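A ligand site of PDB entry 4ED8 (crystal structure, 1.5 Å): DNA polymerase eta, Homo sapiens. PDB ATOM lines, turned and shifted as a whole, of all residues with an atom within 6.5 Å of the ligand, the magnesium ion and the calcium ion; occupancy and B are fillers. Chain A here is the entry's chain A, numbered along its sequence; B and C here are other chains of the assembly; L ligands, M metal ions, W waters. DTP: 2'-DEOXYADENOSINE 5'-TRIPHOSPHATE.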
ATOM      1  N   VAL A  15      20.953  33.187  29.301  1.00  0.00           N
ATOM      2  CA  VAL A  15      19.866  34.030  28.815  1.00  0.00           C
ATOM      3  C   VAL A  15      19.490  33.554  27.409  1.00  0.00           C
ATOM      4  O   VAL A  15      20.359  33.368  26.562  1.00  0.00           O
ATOM      5  CB  VAL A  15      20.317  35.484  28.747  1.00  0.00           C
ATOM      6  CG1 VAL A  15      19.191  36.359  28.189  1.00  0.00           C
ATOM      7  CG2 VAL A  15      20.737  35.965  30.130  1.00  0.00           C
ATOM      8  N   ASP A  16      18.204  33.323  27.182  1.00  0.00           N
ATOM      9  CA  ASP A  16      17.728  32.817  25.905  1.00  0.00           C
ATOM     10  C   ASP A  16      16.538  33.619  25.419  1.00  0.00           C
ATOM     11  O   ASP A  16      15.510  33.707  26.081  1.00  0.00           O
ATOM     12  CB  ASP A  16      17.335  31.358  26.049  1.00  0.00           C
ATOM     13  CG  ASP A  16      16.723  30.804  24.802  1.00  0.00           C
ATOM     14  OD1 ASP A  16      15.506  30.984  24.600  1.00  0.00           O
ATOM     15  OD2 ASP A  16      17.474  30.231  24.007  1.00  0.00           O
ATOM     16  N   MET A  17      16.667  34.239  24.241  1.00  0.00           N
ATOM     17  CA  MET A  17      15.565  35.088  23.771  1.00  0.00           C
ATOM     18  C   MET A  17      14.310  34.270  23.480  1.00  0.00           C
ATOM     19  O   MET A  17      14.389  33.141  23.058  1.00  0.00           O
ATOM     20  CB  MET A  17      15.963  35.827  22.496  1.00  0.00           C
ATOM     21  CG  MET A  17      17.290  36.567  22.564  1.00  0.00           C
ATOM     22  SD  MET A  17      17.356  37.767  23.904  1.00  0.00           S
ATOM     23  CE  MET A  17      16.075  38.896  23.412  1.00  0.00           C
ATOM     24  N   ASP A  18      13.141  34.836  23.761  1.00  0.00           N
ATOM     25  CA  ASP A  18      11.882  34.128  23.486  1.00  0.00           C
ATOM     26  C   ASP A  18      11.573  34.194  22.010  1.00  0.00           C
ATOM     27  O   ASP A  18      11.734  35.248  21.364  1.00  0.00           O
ATOM     28  CB  ASP A  18      10.740  34.724  24.305  1.00  0.00           C
ATOM     29  CG  ASP A  18      10.974  34.628  25.809  1.00  0.00           C
ATOM     30  OD1 ASP A  18      11.631  33.675  26.289  1.00  0.00           O
ATOM     31  OD2 ASP A  18      10.445  35.506  26.507  1.00  0.00           O
ATOM     32  N   CYS A  19      11.160  33.048  21.462  1.00  0.00           N
ATOM     33  CA  CYS A  19      10.827  32.925  20.046  1.00  0.00           C
ATOM     34  C   CYS A  19      11.518  33.966  19.162  1.00  0.00           C
ATOM     35  O   CYS A  19      10.870  34.847  18.558  1.00  0.00           O
ATOM     36  CB  CYS A  19       9.298  33.010  19.813  1.00  0.00           C
ATOM     37  SG  CYS A  19       8.373  34.411  20.563  1.00  0.00           S
ATOM     38  N   PHE A  20      12.837  33.862  19.068  1.00  0.00           N
ATOM     39  CA  PHE A  20      13.636  35.015  18.688  1.00  0.00           C
ATOM     40  C   PHE A  20      13.315  35.590  17.307  1.00  0.00           C
ATOM     41  O   PHE A  20      13.104  36.797  17.182  1.00  0.00           O
ATOM     42  CB  PHE A  20      15.130  34.670  18.800  1.00  0.00           C
ATOM     43  CG  PHE A  20      16.051  35.806  18.490  1.00  0.00           C
ATOM     44  CD1 PHE A  20      15.904  37.048  19.125  1.00  0.00           C
ATOM     45  CD2 PHE A  20      17.078  35.646  17.574  1.00  0.00           C
ATOM     46  CE1 PHE A  20      16.775  38.088  18.832  1.00  0.00           C
ATOM     47  CE2 PHE A  20      17.951  36.701  17.297  1.00  0.00           C
ATOM     48  CZ  PHE A  20      17.805  37.902  17.934  1.00  0.00           C
ATOM     49  N   PHE A  21      13.282  34.749  16.273  1.00  0.00           N
ATOM     50  CA  PHE A  21      13.102  35.316  14.926  1.00  0.00           C
ATOM     51  C   PHE A  21      11.714  35.963  14.836  1.00  0.00           C
ATOM     52  O   PHE A  21      11.538  36.947  14.120  1.00  0.00           O
ATOM     53  CB  PHE A  21      13.257  34.265  13.824  1.00  0.00           C
ATOM     54  CG  PHE A  21      14.672  33.789  13.579  1.00  0.00           C
ATOM     55  CD1 PHE A  21      15.702  34.039  14.481  1.00  0.00           C
ATOM     56  CD2 PHE A  21      14.967  33.105  12.421  1.00  0.00           C
ATOM     57  CE1 PHE A  21      16.995  33.578  14.230  1.00  0.00           C
ATOM     58  CE2 PHE A  21      16.275  32.639  12.155  1.00  0.00           C
ATOM     59  CZ  PHE A  21      17.275  32.879  13.064  1.00  0.00           C
ATOM     60  N   VAL A  22      10.739  35.400  15.546  1.00  0.00           N
ATOM     61  CA  VAL A  22       9.393  36.007  15.584  1.00  0.00           C
ATOM     62  C   VAL A  22       9.434  37.405  16.217  1.00  0.00           C
ATOM     63  O   VAL A  22       8.855  38.346  15.675  1.00  0.00           O
ATOM     64  CB  VAL A  22       8.412  35.104  16.346  1.00  0.00           C
ATOM     65  CG1 VAL A  22       7.138  35.872  16.733  1.00  0.00           C
ATOM     66  CG2 VAL A  22       8.093  33.883  15.497  1.00  0.00           C
ATOM     67  N   GLN A  41      10.581  29.834   6.002  1.00  0.00           N
ATOM     68  CA  GLN A  41      11.687  29.864   5.059  1.00  0.00           C
ATOM     69  C   GLN A  41      11.202  29.250   3.761  1.00  0.00           C
ATOM     70  O   GLN A  41      10.795  28.089   3.747  1.00  0.00           O
ATOM     71  CB  GLN A  41      12.812  29.009   5.641  1.00  0.00           C
ATOM     72  CG  GLN A  41      14.194  29.323   5.181  1.00  0.00           C
ATOM     73  CD  GLN A  41      15.228  28.841   6.201  1.00  0.00           C
ATOM     74  OE1 GLN A  41      16.114  29.596   6.603  1.00  0.00           O
ATOM     75  NE2 GLN A  41      15.135  27.570   6.612  1.00  0.00           N
ATOM     76  N   ILE A  51      10.377  27.985  11.015  1.00  0.00           N
ATOM     77  CA  ILE A  51      11.570  27.903  11.853  1.00  0.00           C
ATOM     78  C   ILE A  51      11.434  28.601  13.212  1.00  0.00           C
ATOM     79  O   ILE A  51      12.295  28.436  14.064  1.00  0.00           O
ATOM     80  CB  ILE A  51      12.836  28.356  11.112  1.00  0.00           C
ATOM     81  CG1 ILE A  51      12.762  29.802  10.663  1.00  0.00           C
ATOM     82  CG2 ILE A  51      13.100  27.440   9.916  1.00  0.00           C
ATOM     83  CD1 ILE A  51      14.098  30.324  10.178  1.00  0.00           C
ATOM     84  N   ALA A  52      10.356  29.335  13.432  1.00  0.00           N
ATOM     85  CA  ALA A  52      10.115  29.977  14.724  1.00  0.00           C
ATOM     86  C   ALA A  52       8.634  30.266  14.889  1.00  0.00           C
ATOM     87  O   ALA A  52       7.958  30.557  13.901  1.00  0.00           O
ATOM     88  CB  ALA A  52      10.943  31.261  14.868  1.00  0.00           C
ATOM     89  N   VAL A  53       8.132  30.188  16.128  1.00  0.00           N
ATOM     90  CA  VAL A  53       6.692  30.212  16.389  1.00  0.00           C
ATOM     91  C   VAL A  53       6.380  31.026  17.645  1.00  0.00           C
ATOM     92  O   VAL A  53       6.985  30.799  18.688  1.00  0.00           O
ATOM     93  CB  VAL A  53       6.178  28.763  16.604  1.00  0.00           C
ATOM     94  CG1 VAL A  53       4.660  28.767  16.774  1.00  0.00           C
ATOM     95  CG2 VAL A  53       6.587  27.873  15.447  1.00  0.00           C
ATOM     96  N   TYR A  55       4.331  32.339  20.947  1.00  0.00           N
ATOM     97  CA  TYR A  55       3.663  31.561  21.996  1.00  0.00           C
ATOM     98  C   TYR A  55       2.151  31.449  21.769  1.00  0.00           C
ATOM     99  O   TYR A  55       1.556  30.408  22.069  1.00  0.00           O
ATOM    100  CB  TYR A  55       4.043  32.091  23.395  1.00  0.00           C
ATOM    101  CG  TYR A  55       5.427  31.604  23.780  1.00  0.00           C
ATOM    102  CD1 TYR A  55       6.570  32.224  23.283  1.00  0.00           C
ATOM    103  CD2 TYR A  55       5.580  30.471  24.569  1.00  0.00           C
ATOM    104  CE1 TYR A  55       7.835  31.749  23.590  1.00  0.00           C
ATOM    105  CE2 TYR A  55       6.846  29.994  24.890  1.00  0.00           C
ATOM    106  CZ  TYR A  55       7.970  30.629  24.389  1.00  0.00           C
ATOM    107  OH  TYR A  55       9.209  30.136  24.723  1.00  0.00           O
ATOM    108  N   ARG A  58       1.825  28.624  19.362  1.00  0.00           N
ATOM    109  CA  ARG A  58       2.148  27.338  19.976  1.00  0.00           C
ATOM    110  C   ARG A  58       0.934  26.733  20.672  1.00  0.00           C
ATOM    111  O   ARG A  58       0.784  25.500  20.727  1.00  0.00           O
ATOM    112  CB  ARG A  58       3.303  27.462  20.968  1.00  0.00           C
ATOM    113  CG  ARG A  58       4.615  27.828  20.312  1.00  0.00           C
ATOM    114  CD  ARG A  58       5.718  27.980  21.353  1.00  0.00           C
ATOM    115  NE  ARG A  58       6.847  28.712  20.781  1.00  0.00           N
ATOM    116  CZ  ARG A  58       8.072  28.731  21.281  1.00  0.00           C
ATOM    117  NH1 ARG A  58       8.369  28.028  22.374  1.00  0.00           N
ATOM    118  NH2 ARG A  58       9.019  29.443  20.666  1.00  0.00           N
ATOM    119  N   ARG A  64       7.999  24.418  15.301  1.00  0.00           N
ATOM    120  CA  ARG A  64       9.139  24.425  14.410  1.00  0.00           C
ATOM    121  C   ARG A  64       9.190  23.114  13.620  1.00  0.00           C
ATOM    122  O   ARG A  64       8.797  22.050  14.134  1.00  0.00           O
ATOM    123  CB  ARG A  64      10.410  24.635  15.229  1.00  0.00           C
ATOM    124  CG  ARG A  64      11.701  24.239  14.551  1.00  0.00           C
ATOM    125  CD  ARG A  64      12.884  24.645  15.424  1.00  0.00           C
ATOM    126  NE  ARG A  64      12.826  26.075  15.688  1.00  0.00           N
ATOM    127  CZ  ARG A  64      13.015  26.649  16.875  1.00  0.00           C
ATOM    128  NH1 ARG A  64      13.300  25.926  17.951  1.00  0.00           N
ATOM    129  NH2 ARG A  64      12.917  27.972  16.968  1.00  0.00           N
ATOM    130  N   LEU A  92      20.059  35.099   6.454  1.00  0.00           N
ATOM    131  CA  LEU A  92      19.729  35.301   7.867  1.00  0.00           C
ATOM    132  C   LEU A  92      20.294  36.581   8.512  1.00  0.00           C
ATOM    133  O   LEU A  92      20.275  36.727   9.742  1.00  0.00           O
ATOM    134  CB  LEU A  92      20.169  34.083   8.707  1.00  0.00           C
ATOM    135  CG  LEU A  92      19.631  32.751   8.168  1.00  0.00           C
ATOM    136  CD1 LEU A  92      20.233  31.594   8.944  1.00  0.00           C
ATOM    137  CD2 LEU A  92      18.106  32.729   8.277  1.00  0.00           C
ATOM    138  N   SER A 116      24.630  30.511  20.902  1.00  0.00           N
ATOM    139  CA  SER A 116      23.888  30.376  19.650  1.00  0.00           C
ATOM    140  C   SER A 116      23.457  31.765  19.228  1.00  0.00           C
ATOM    141  O   SER A 116      23.822  32.748  19.848  1.00  0.00           O
ATOM    142  CB  SER A 116      22.663  29.486  19.827  1.00  0.00           C
ATOM    143  OG  SER A 116      21.619  30.181  20.483  1.00  0.00           O
ATOM    144  N   ILE A 117      22.679  31.833  18.157  1.00  0.00           N
ATOM    145  CA  ILE A 117      22.224  33.125  17.650  1.00  0.00           C
ATOM    146  C   ILE A 117      21.416  33.891  18.711  1.00  0.00           C
ATOM    147  O   ILE A 117      21.384  35.121  18.702  1.00  0.00           O
ATOM    148  CB  ILE A 117      21.429  32.964  16.333  1.00  0.00           C
ATOM    149  CG1 ILE A 117      21.285  34.305  15.602  1.00  0.00           C
ATOM    150  CG2 ILE A 117      20.069  32.312  16.593  1.00  0.00           C
ATOM    151  CD1 ILE A 117      20.891  34.172  14.145  1.00  0.00           C
ATOM    152  N   ASP A 118      20.761  33.177  19.625  1.00  0.00           N
ATOM    153  CA  ASP A 118      19.923  33.878  20.579  1.00  0.00           C
ATOM    154  C   ASP A 118      20.149  33.533  22.027  1.00  0.00           C
ATOM    155  O   ASP A 118      19.288  33.788  22.883  1.00  0.00           O
ATOM    156  CB  ASP A 118      18.448  33.687  20.218  1.00  0.00           C
ATOM    157  CG  ASP A 118      17.869  32.418  20.791  1.00  0.00           C
ATOM    158  OD1 ASP A 118      16.677  32.486  21.181  1.00  0.00           O
ATOM    159  OD2 ASP A 118      18.584  31.376  20.890  1.00  0.00           O
ATOM    160  N   GLU A 119      21.315  32.988  22.329  1.00  0.00           N
ATOM    161  CA  GLU A 119      21.579  32.740  23.717  1.00  0.00           C
ATOM    162  C   GLU A 119      23.012  32.843  24.119  1.00  0.00           C
ATOM    163  O   GLU A 119      23.900  32.619  23.316  1.00  0.00           O
ATOM    164  CB  GLU A 119      21.000  31.397  24.152  1.00  0.00           C
ATOM    165  CG  GLU A 119      21.651  30.215  23.519  1.00  0.00           C
ATOM    166  CD  GLU A 119      20.784  28.972  23.583  1.00  0.00           C
ATOM    167  OE1 GLU A 119      20.753  28.304  24.641  1.00  0.00           O
ATOM    168  OE2 GLU A 119      20.105  28.673  22.583  1.00  0.00           O
ATOM    169  N   SER A 216      14.077  34.799  28.439  1.00  0.00           N
ATOM    170  CA  SER A 216      14.012  34.040  29.680  1.00  0.00           C
ATOM    171  C   SER A 216      15.445  33.790  30.131  1.00  0.00           C
ATOM    172  O   SER A 216      16.377  33.980  29.356  1.00  0.00           O
ATOM    173  CB  SER A 216      13.278  32.715  29.460  1.00  0.00           C
ATOM    174  OG  SER A 216      11.939  32.978  29.048  1.00  0.00           O
ATOM    175  N   LYS A 227      21.103  26.306  31.884  1.00  0.00           N
ATOM    176  CA  LYS A 227      20.341  26.023  30.669  1.00  0.00           C
ATOM    177  C   LYS A 227      19.035  25.290  31.001  1.00  0.00           C
ATOM    178  O   LYS A 227      17.957  25.665  30.505  1.00  0.00           O
ATOM    179  CB  LYS A 227      21.201  25.199  29.690  1.00  0.00           C
ATOM    180  CG  LYS A 227      20.505  24.820  28.387  1.00  0.00           C
ATOM    181  CD  LYS A 227      20.082  26.029  27.559  1.00  0.00           C
ATOM    182  CE  LYS A 227      19.545  25.593  26.203  1.00  0.00           C
ATOM    183  NZ  LYS A 227      18.742  26.654  25.525  1.00  0.00           N
ATOM    184  N   LYS A 234       9.136  29.547  30.788  1.00  0.00           N
ATOM    185  CA  LYS A 234       9.186  30.393  29.611  1.00  0.00           C
ATOM    186  C   LYS A 234       7.746  30.714  29.249  1.00  0.00           C
ATOM    187  O   LYS A 234       6.845  29.934  29.552  1.00  0.00           O
ATOM    188  CB  LYS A 234       9.880  29.673  28.441  1.00  0.00           C
ATOM    189  CG  LYS A 234      11.405  29.898  28.339  1.00  0.00           C
ATOM    190  CD  LYS A 234      11.913  29.647  26.888  1.00  0.00           C
ATOM    191  CE  LYS A 234      13.309  30.255  26.619  1.00  0.00           C
ATOM    192  NZ  LYS A 234      13.295  31.492  25.730  1.00  0.00           N
ATOM    193  N   PRO A 235       7.514  31.858  28.609  1.00  0.00           N
ATOM    194  CA  PRO A 235       8.501  32.876  28.249  1.00  0.00           C
ATOM    195  C   PRO A 235       8.531  34.033  29.241  1.00  0.00           C
ATOM    196  O   PRO A 235       7.691  34.103  30.148  1.00  0.00           O
ATOM    197  CB  PRO A 235       7.951  33.388  26.921  1.00  0.00           C
ATOM    198  CG  PRO A 235       6.459  33.345  27.118  1.00  0.00           C
ATOM    199  CD  PRO A 235       6.202  32.124  27.981  1.00  0.00           C
ATOM    200  P    DA B   9      19.078  23.458  21.812  1.00  0.00           P
ATOM    201  OP1  DA B   9      18.592  24.113  23.040  1.00  0.00           O
ATOM    202  OP2  DA B   9      18.216  22.489  21.107  1.00  0.00           O
ATOM    203  O5'  DA B   9      19.478  24.615  20.782  1.00  0.00           O
ATOM    204  C5'  DA B   9      20.365  25.680  21.149  1.00  0.00           C
ATOM    205  C4'  DA B   9      20.292  26.721  20.064  1.00  0.00           C
ATOM    206  O4'  DA B   9      20.734  26.043  18.871  1.00  0.00           O
ATOM    207  C3'  DA B   9      18.847  27.147  19.831  1.00  0.00           C
ATOM    208  O3'  DA B   9      18.726  28.550  20.002  1.00  0.00           O
ATOM    209  C2'  DA B   9      18.531  26.750  18.398  1.00  0.00           C
ATOM    210  C1'  DA B   9      19.874  26.380  17.785  1.00  0.00           C
ATOM    211  N9   DA B   9      19.790  25.212  16.916  1.00  0.00           N
ATOM    212  C8   DA B   9      19.610  23.916  17.285  1.00  0.00           C
ATOM    213  N7   DA B   9      19.578  23.071  16.280  1.00  0.00           N
ATOM    214  C5   DA B   9      19.739  23.880  15.156  1.00  0.00           C
ATOM    215  C6   DA B   9      19.801  23.604  13.775  1.00  0.00           C
ATOM    216  N6   DA B   9      19.698  22.372  13.263  1.00  0.00           N
ATOM    217  N1   DA B   9      19.973  24.648  12.942  1.00  0.00           N
ATOM    218  C2   DA B   9      20.073  25.885  13.463  1.00  0.00           C
ATOM    219  N3   DA B   9      20.047  26.265  14.741  1.00  0.00           N
ATOM    220  C4   DA B   9      19.875  25.203  15.536  1.00  0.00           C
ATOM    221  P    DA C   2      10.467  16.095   5.615  1.00  0.00           P
ATOM    222  OP1  DA C   2      10.133  16.813   4.362  1.00  0.00           O
ATOM    223  OP2  DA C   2      11.628  15.180   5.665  1.00  0.00           O
ATOM    224  O5'  DA C   2      10.645  17.164   6.794  1.00  0.00           O
ATOM    225  C5'  DA C   2      11.914  17.775   6.998  1.00  0.00           C
ATOM    226  C4'  DA C   2      11.794  19.286   6.976  1.00  0.00           C
ATOM    227  O4'  DA C   2      11.348  19.763   8.270  1.00  0.00           O
ATOM    228  C3'  DA C   2      13.099  20.018   6.694  1.00  0.00           C
ATOM    229  O3'  DA C   2      13.150  20.275   5.319  1.00  0.00           O
ATOM    230  C2'  DA C   2      12.969  21.328   7.466  1.00  0.00           C
ATOM    231  C1'  DA C   2      12.030  20.948   8.608  1.00  0.00           C
ATOM    232  N9   DA C   2      12.712  20.758   9.881  1.00  0.00           N
ATOM    233  C8   DA C   2      13.119  19.572  10.427  1.00  0.00           C
ATOM    234  N7   DA C   2      13.711  19.711  11.595  1.00  0.00           N
ATOM    235  C5   DA C   2      13.685  21.084  11.820  1.00  0.00           C
ATOM    236  C6   DA C   2      14.148  21.892  12.875  1.00  0.00           C
ATOM    237  N6   DA C   2      14.762  21.400  13.966  1.00  0.00           N
ATOM    238  N1   DA C   2      13.960  23.221  12.781  1.00  0.00           N
ATOM    239  C2   DA C   2      13.343  23.718  11.698  1.00  0.00           C
ATOM    240  N3   DA C   2      12.862  23.065  10.637  1.00  0.00           N
ATOM    241  C4   DA C   2      13.070  21.740  10.774  1.00  0.00           C
ATOM    242  P    DT C   3      14.526  20.122   4.506  1.00  0.00           P
ATOM    243  OP1  DT C   3      14.185  19.830   3.096  1.00  0.00           O
ATOM    244  OP2  DT C   3      15.412  19.217   5.266  1.00  0.00           O
ATOM    245  O5'  DT C   3      15.177  21.581   4.585  1.00  0.00           O
ATOM    246  C5'  DT C   3      14.534  22.700   3.992  1.00  0.00           C
ATOM    247  C4'  DT C   3      15.340  23.954   4.284  1.00  0.00           C
ATOM    248  O4'  DT C   3      15.389  24.152   5.719  1.00  0.00           O
ATOM    249  C3'  DT C   3      16.793  23.955   3.826  1.00  0.00           C
ATOM    250  O3'  DT C   3      17.070  25.283   3.449  1.00  0.00           O
ATOM    251  C2'  DT C   3      17.555  23.519   5.074  1.00  0.00           C
ATOM    252  C1'  DT C   3      16.736  24.201   6.160  1.00  0.00           C
ATOM    253  N1   DT C   3      16.755  23.553   7.497  1.00  0.00           N
ATOM    254  C2   DT C   3      16.735  24.405   8.578  1.00  0.00           C
ATOM    255  O2   DT C   3      16.724  25.622   8.473  1.00  0.00           O
ATOM    256  N3   DT C   3      16.722  23.778   9.791  1.00  0.00           N
ATOM    257  C4   DT C   3      16.725  22.425  10.042  1.00  0.00           C
ATOM    258  O4   DT C   3      16.727  21.981  11.195  1.00  0.00           O
ATOM    259  C5   DT C   3      16.740  21.587   8.864  1.00  0.00           C
ATOM    260  C7   DT C   3      16.743  20.095   9.016  1.00  0.00           C
ATOM    261  C6   DT C   3      16.737  22.180   7.654  1.00  0.00           C
ATOM    262  P    DT C   4      18.510  25.685   2.855  1.00  0.00           P
ATOM    263  OP1  DT C   4      18.284  26.672   1.770  1.00  0.00           O
ATOM    264  OP2  DT C   4      19.275  24.446   2.587  1.00  0.00           O
ATOM    265  O5'  DT C   4      19.212  26.425   4.080  1.00  0.00           O
ATOM    266  C5'  DT C   4      18.670  27.666   4.580  1.00  0.00           C
ATOM    267  C4'  DT C   4      19.462  28.143   5.770  1.00  0.00           C
ATOM    268  O4'  DT C   4      19.207  27.258   6.881  1.00  0.00           O
ATOM    269  C3'  DT C   4      20.979  28.183   5.571  1.00  0.00           C
ATOM    270  O3'  DT C   4      21.487  29.360   6.197  1.00  0.00           O
ATOM    271  C2'  DT C   4      21.450  26.915   6.281  1.00  0.00           C
ATOM    272  C1'  DT C   4      20.462  26.910   7.464  1.00  0.00           C
ATOM    273  N1   DT C   4      20.339  25.620   8.175  1.00  0.00           N
ATOM    274  C2   DT C   4      20.173  25.651   9.547  1.00  0.00           C
ATOM    275  O2   DT C   4      20.118  26.667  10.224  1.00  0.00           O
ATOM    276  N3   DT C   4      20.079  24.437  10.145  1.00  0.00           N
ATOM    277  C4   DT C   4      20.115  23.207   9.546  1.00  0.00           C
ATOM    278  O4   DT C   4      20.004  22.184  10.215  1.00  0.00           O
ATOM    279  C5   DT C   4      20.280  23.220   8.109  1.00  0.00           C
ATOM    280  C7   DT C   4      20.321  21.904   7.368  1.00  0.00           C
ATOM    281  C6   DT C   4      20.375  24.412   7.500  1.00  0.00           C
HETATM  282  PG  DTP L   1      12.005  29.714  22.530  1.00  0.00           P
HETATM  283  O1G DTP L   1      11.455  28.326  22.792  1.00  0.00           O
HETATM  284  O2G DTP L   1      11.149  30.796  23.073  1.00  0.00           O
HETATM  285  O3G DTP L   1      13.481  29.826  22.830  1.00  0.00           O
HETATM  286  PB  DTP L   1      13.046  30.223  19.877  1.00  0.00           P
HETATM  287  O1B DTP L   1      13.915  31.355  20.370  1.00  0.00           O
HETATM  288  O2B DTP L   1      12.363  30.399  18.538  1.00  0.00           O
HETATM  289  O3B DTP L   1      11.865  29.872  20.922  1.00  0.00           O
HETATM  290  PA  DTP L   1      15.462  28.597  19.908  1.00  0.00           P
HETATM  291  O1A DTP L   1      15.649  27.094  19.813  1.00  0.00           O
HETATM  292  O2A DTP L   1      16.074  29.275  21.101  1.00  0.00           O
HETATM  293  O3A DTP L   1      13.853  28.837  19.844  1.00  0.00           O
HETATM  294  O5' DTP L   1      16.089  29.176  18.547  1.00  0.00           O
HETATM  295  C5' DTP L   1      16.482  30.534  18.368  1.00  0.00           C
HETATM  296  C4' DTP L   1      16.257  30.920  16.919  1.00  0.00           C
HETATM  297  O4' DTP L   1      17.097  30.148  16.048  1.00  0.00           O
HETATM  298  C3' DTP L   1      14.835  30.657  16.437  1.00  0.00           C
HETATM  299  O3' DTP L   1      13.960  31.765  16.671  1.00  0.00           O
HETATM  300  C2' DTP L   1      15.008  30.370  14.956  1.00  0.00           C
HETATM  301  C1' DTP L   1      16.386  29.730  14.876  1.00  0.00           C
HETATM  302  N9  DTP L   1      16.342  28.247  14.867  1.00  0.00           N
HETATM  303  C8  DTP L   1      16.221  27.429  15.938  1.00  0.00           C
HETATM  304  N7  DTP L   1      16.268  26.151  15.511  1.00  0.00           N
HETATM  305  C5  DTP L   1      16.419  26.165  14.167  1.00  0.00           C
HETATM  306  C6  DTP L   1      16.529  25.188  13.199  1.00  0.00           C
HETATM  307  N6  DTP L   1      16.485  23.874  13.544  1.00  0.00           N
HETATM  308  N1  DTP L   1      16.694  25.546  11.904  1.00  0.00           N
HETATM  309  C2  DTP L   1      16.732  26.848  11.564  1.00  0.00           C
HETATM  310  N3  DTP L   1      16.639  27.818  12.480  1.00  0.00           N
HETATM  311  C4  DTP L   1      16.478  27.495  13.780  1.00  0.00           C
HETATM  312 MG    MG M   1      18.152  29.323  22.117  1.00  0.00          MG
HETATM  313 CA    CA M   2      15.213  31.162  22.238  1.00  0.00          CA
HETATM  314  O   HOH W   1      16.242  24.773  17.991  1.00  0.00           O
HETATM  315  O   HOH W   2      14.451  27.386  23.725  1.00  0.00           O
HETATM  316  O   HOH W   3      17.166  27.621  23.023  1.00  0.00           O
HETATM  317  O   HOH W   4      10.046  29.299  18.000  1.00  0.00           O
HETATM  318  O   HOH W   5      18.039  30.005  11.248  1.00  0.00           O
HETATM  319  O   HOH W   6      19.874  29.056  14.918  1.00  0.00           O
HETATM  320  O   HOH W   7      11.348  26.225  21.176  1.00  0.00           O
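O2G of the ligand is in hydrogen-bond range of OH of Tyr 55, 2.6 Å away. N1 of DA 2 of chain C lies within hydrogen-bond range of a nitrogen (N6) of the ligand (2.7 Å). O4 of DT 3 of chain C is in hydrogen-bond range of a nitrogen (N6) of the ligand (3.0 Å). N of Cys 19 is in hydrogen-bond range of O2G of the ligand. The guanidinium group (NH1) of Arg 58 lies within salt-bridge range of an oxygen (O1G) of the ligand, at 3.1 Å. An oxygen (O2B) of the ligand is in salt-bridge range of the guanidinium group (NH2) of Arg 64, 2.9 Å away. The backbone NH (N) of Phe 20 sits at hydrogen-bond distance from an oxygen (O3') of the ligand. N of Phe 21 lies within hydrogen-bond range of O3' of the ligand (3.1 Å). An oxygen (O2G) of the ligand lies within salt-bridge range of the side-chain amino group (NZ) of Lys 234.
Water W1 lies within hydrogen-bond range of N7 of the ligand (2.8 Å) and NH1 of Arg 64 (3.2 Å). Water W6 bridges N3 of DA 9 of chain B (2.8 Å) and O4' of the ligand (3.2 Å).
O of Asp 16 is in hydrogen-bond range of NZ of Lys 234, 3.2 Å away. The side-chain hydroxyl (OG) of Ser 116 lies close to the backbone NH (N) of Asp 118, 3.2 Å away. The backbone carbonyl oxygen of Met 17 lies close to the side-chain amino group of Lys 234 (3.3 Å). The side-chain hydroxyl (OG) of Ser 116 lies close to O3' of DA 9 of chain B, at 3.4 Å. NH1 of Arg 58 lies within hydrogen-bond range of OH of Tyr 55, 3.3 Å away. The guanidinium group (NE) of Arg 64 lies within hydrogen-bond range of the backbone carbonyl oxygen (O) of Ile 51, 2.9 Å away. The side-chain amino group (NZ) of Lys 234 is in salt-bridge range of the side-chain carboxylate (OD1) of Asp 18. OD1 of Asp 18 lies within hydrogen-bond range of OG of Ser 216, at 2.9 Å.
Lys 234 touches the calcium ion. Of the 28 residues printed, 4 come within 4 Å of the calcium ion.
Asp 18 touches the ligand. Ile 51 touches the ligand. Ala 52 touches the ligand (CB to O3', 3.6 Å). CG2 of Ile 117 touches O4' of the ligand, at 3.7 Å. DT 4 of chain C touches the ligand (O2 to C2, 3.6 Å). Hydrophobic or aromatic side chains within 4 Å of the ligand: Phe 20, Phe 21, Ala 52, Tyr 55 and Ile 117. Of the 28 residues printed, 18 come within 4 Å of the ligand. Along chain A the residues within 4 Å of the ligand span positions 16 to 234.
The calcium ion is bound by OD1 of Asp 118 (2.2 Å), O3G of the ligand (2.3 Å), O1B of the ligand (2.3 Å), O of Met 17 (2.3 Å), O2A of the ligand (2.4 Å) and OD1 of Asp 16 (2.4 Å). The calcium ion has six donor atoms within binding distance. Slightly farther from the calcium ion lies OD2 of Asp 16 (3.0 Å).
Merely in contact with the magnesium ion: Ser 116. Of the 28 residues printed, 5 come within 4 Å of the magnesium ion. The nearest printed residue that does not touch the magnesium ion is Lys 227 (4.4 Å).
The magnesium ion is bound by OE2 of Glu 119 (2.1 Å), water W3 (2.2 Å), OD2 of Asp 16 (2.2 Å), O2A of the ligand (2.3 Å), O3' of DA 9 of chain B (2.3 Å) and OD2 of Asp 118 (2.4 Å). The magnesium ion has six donor atoms within binding distance.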
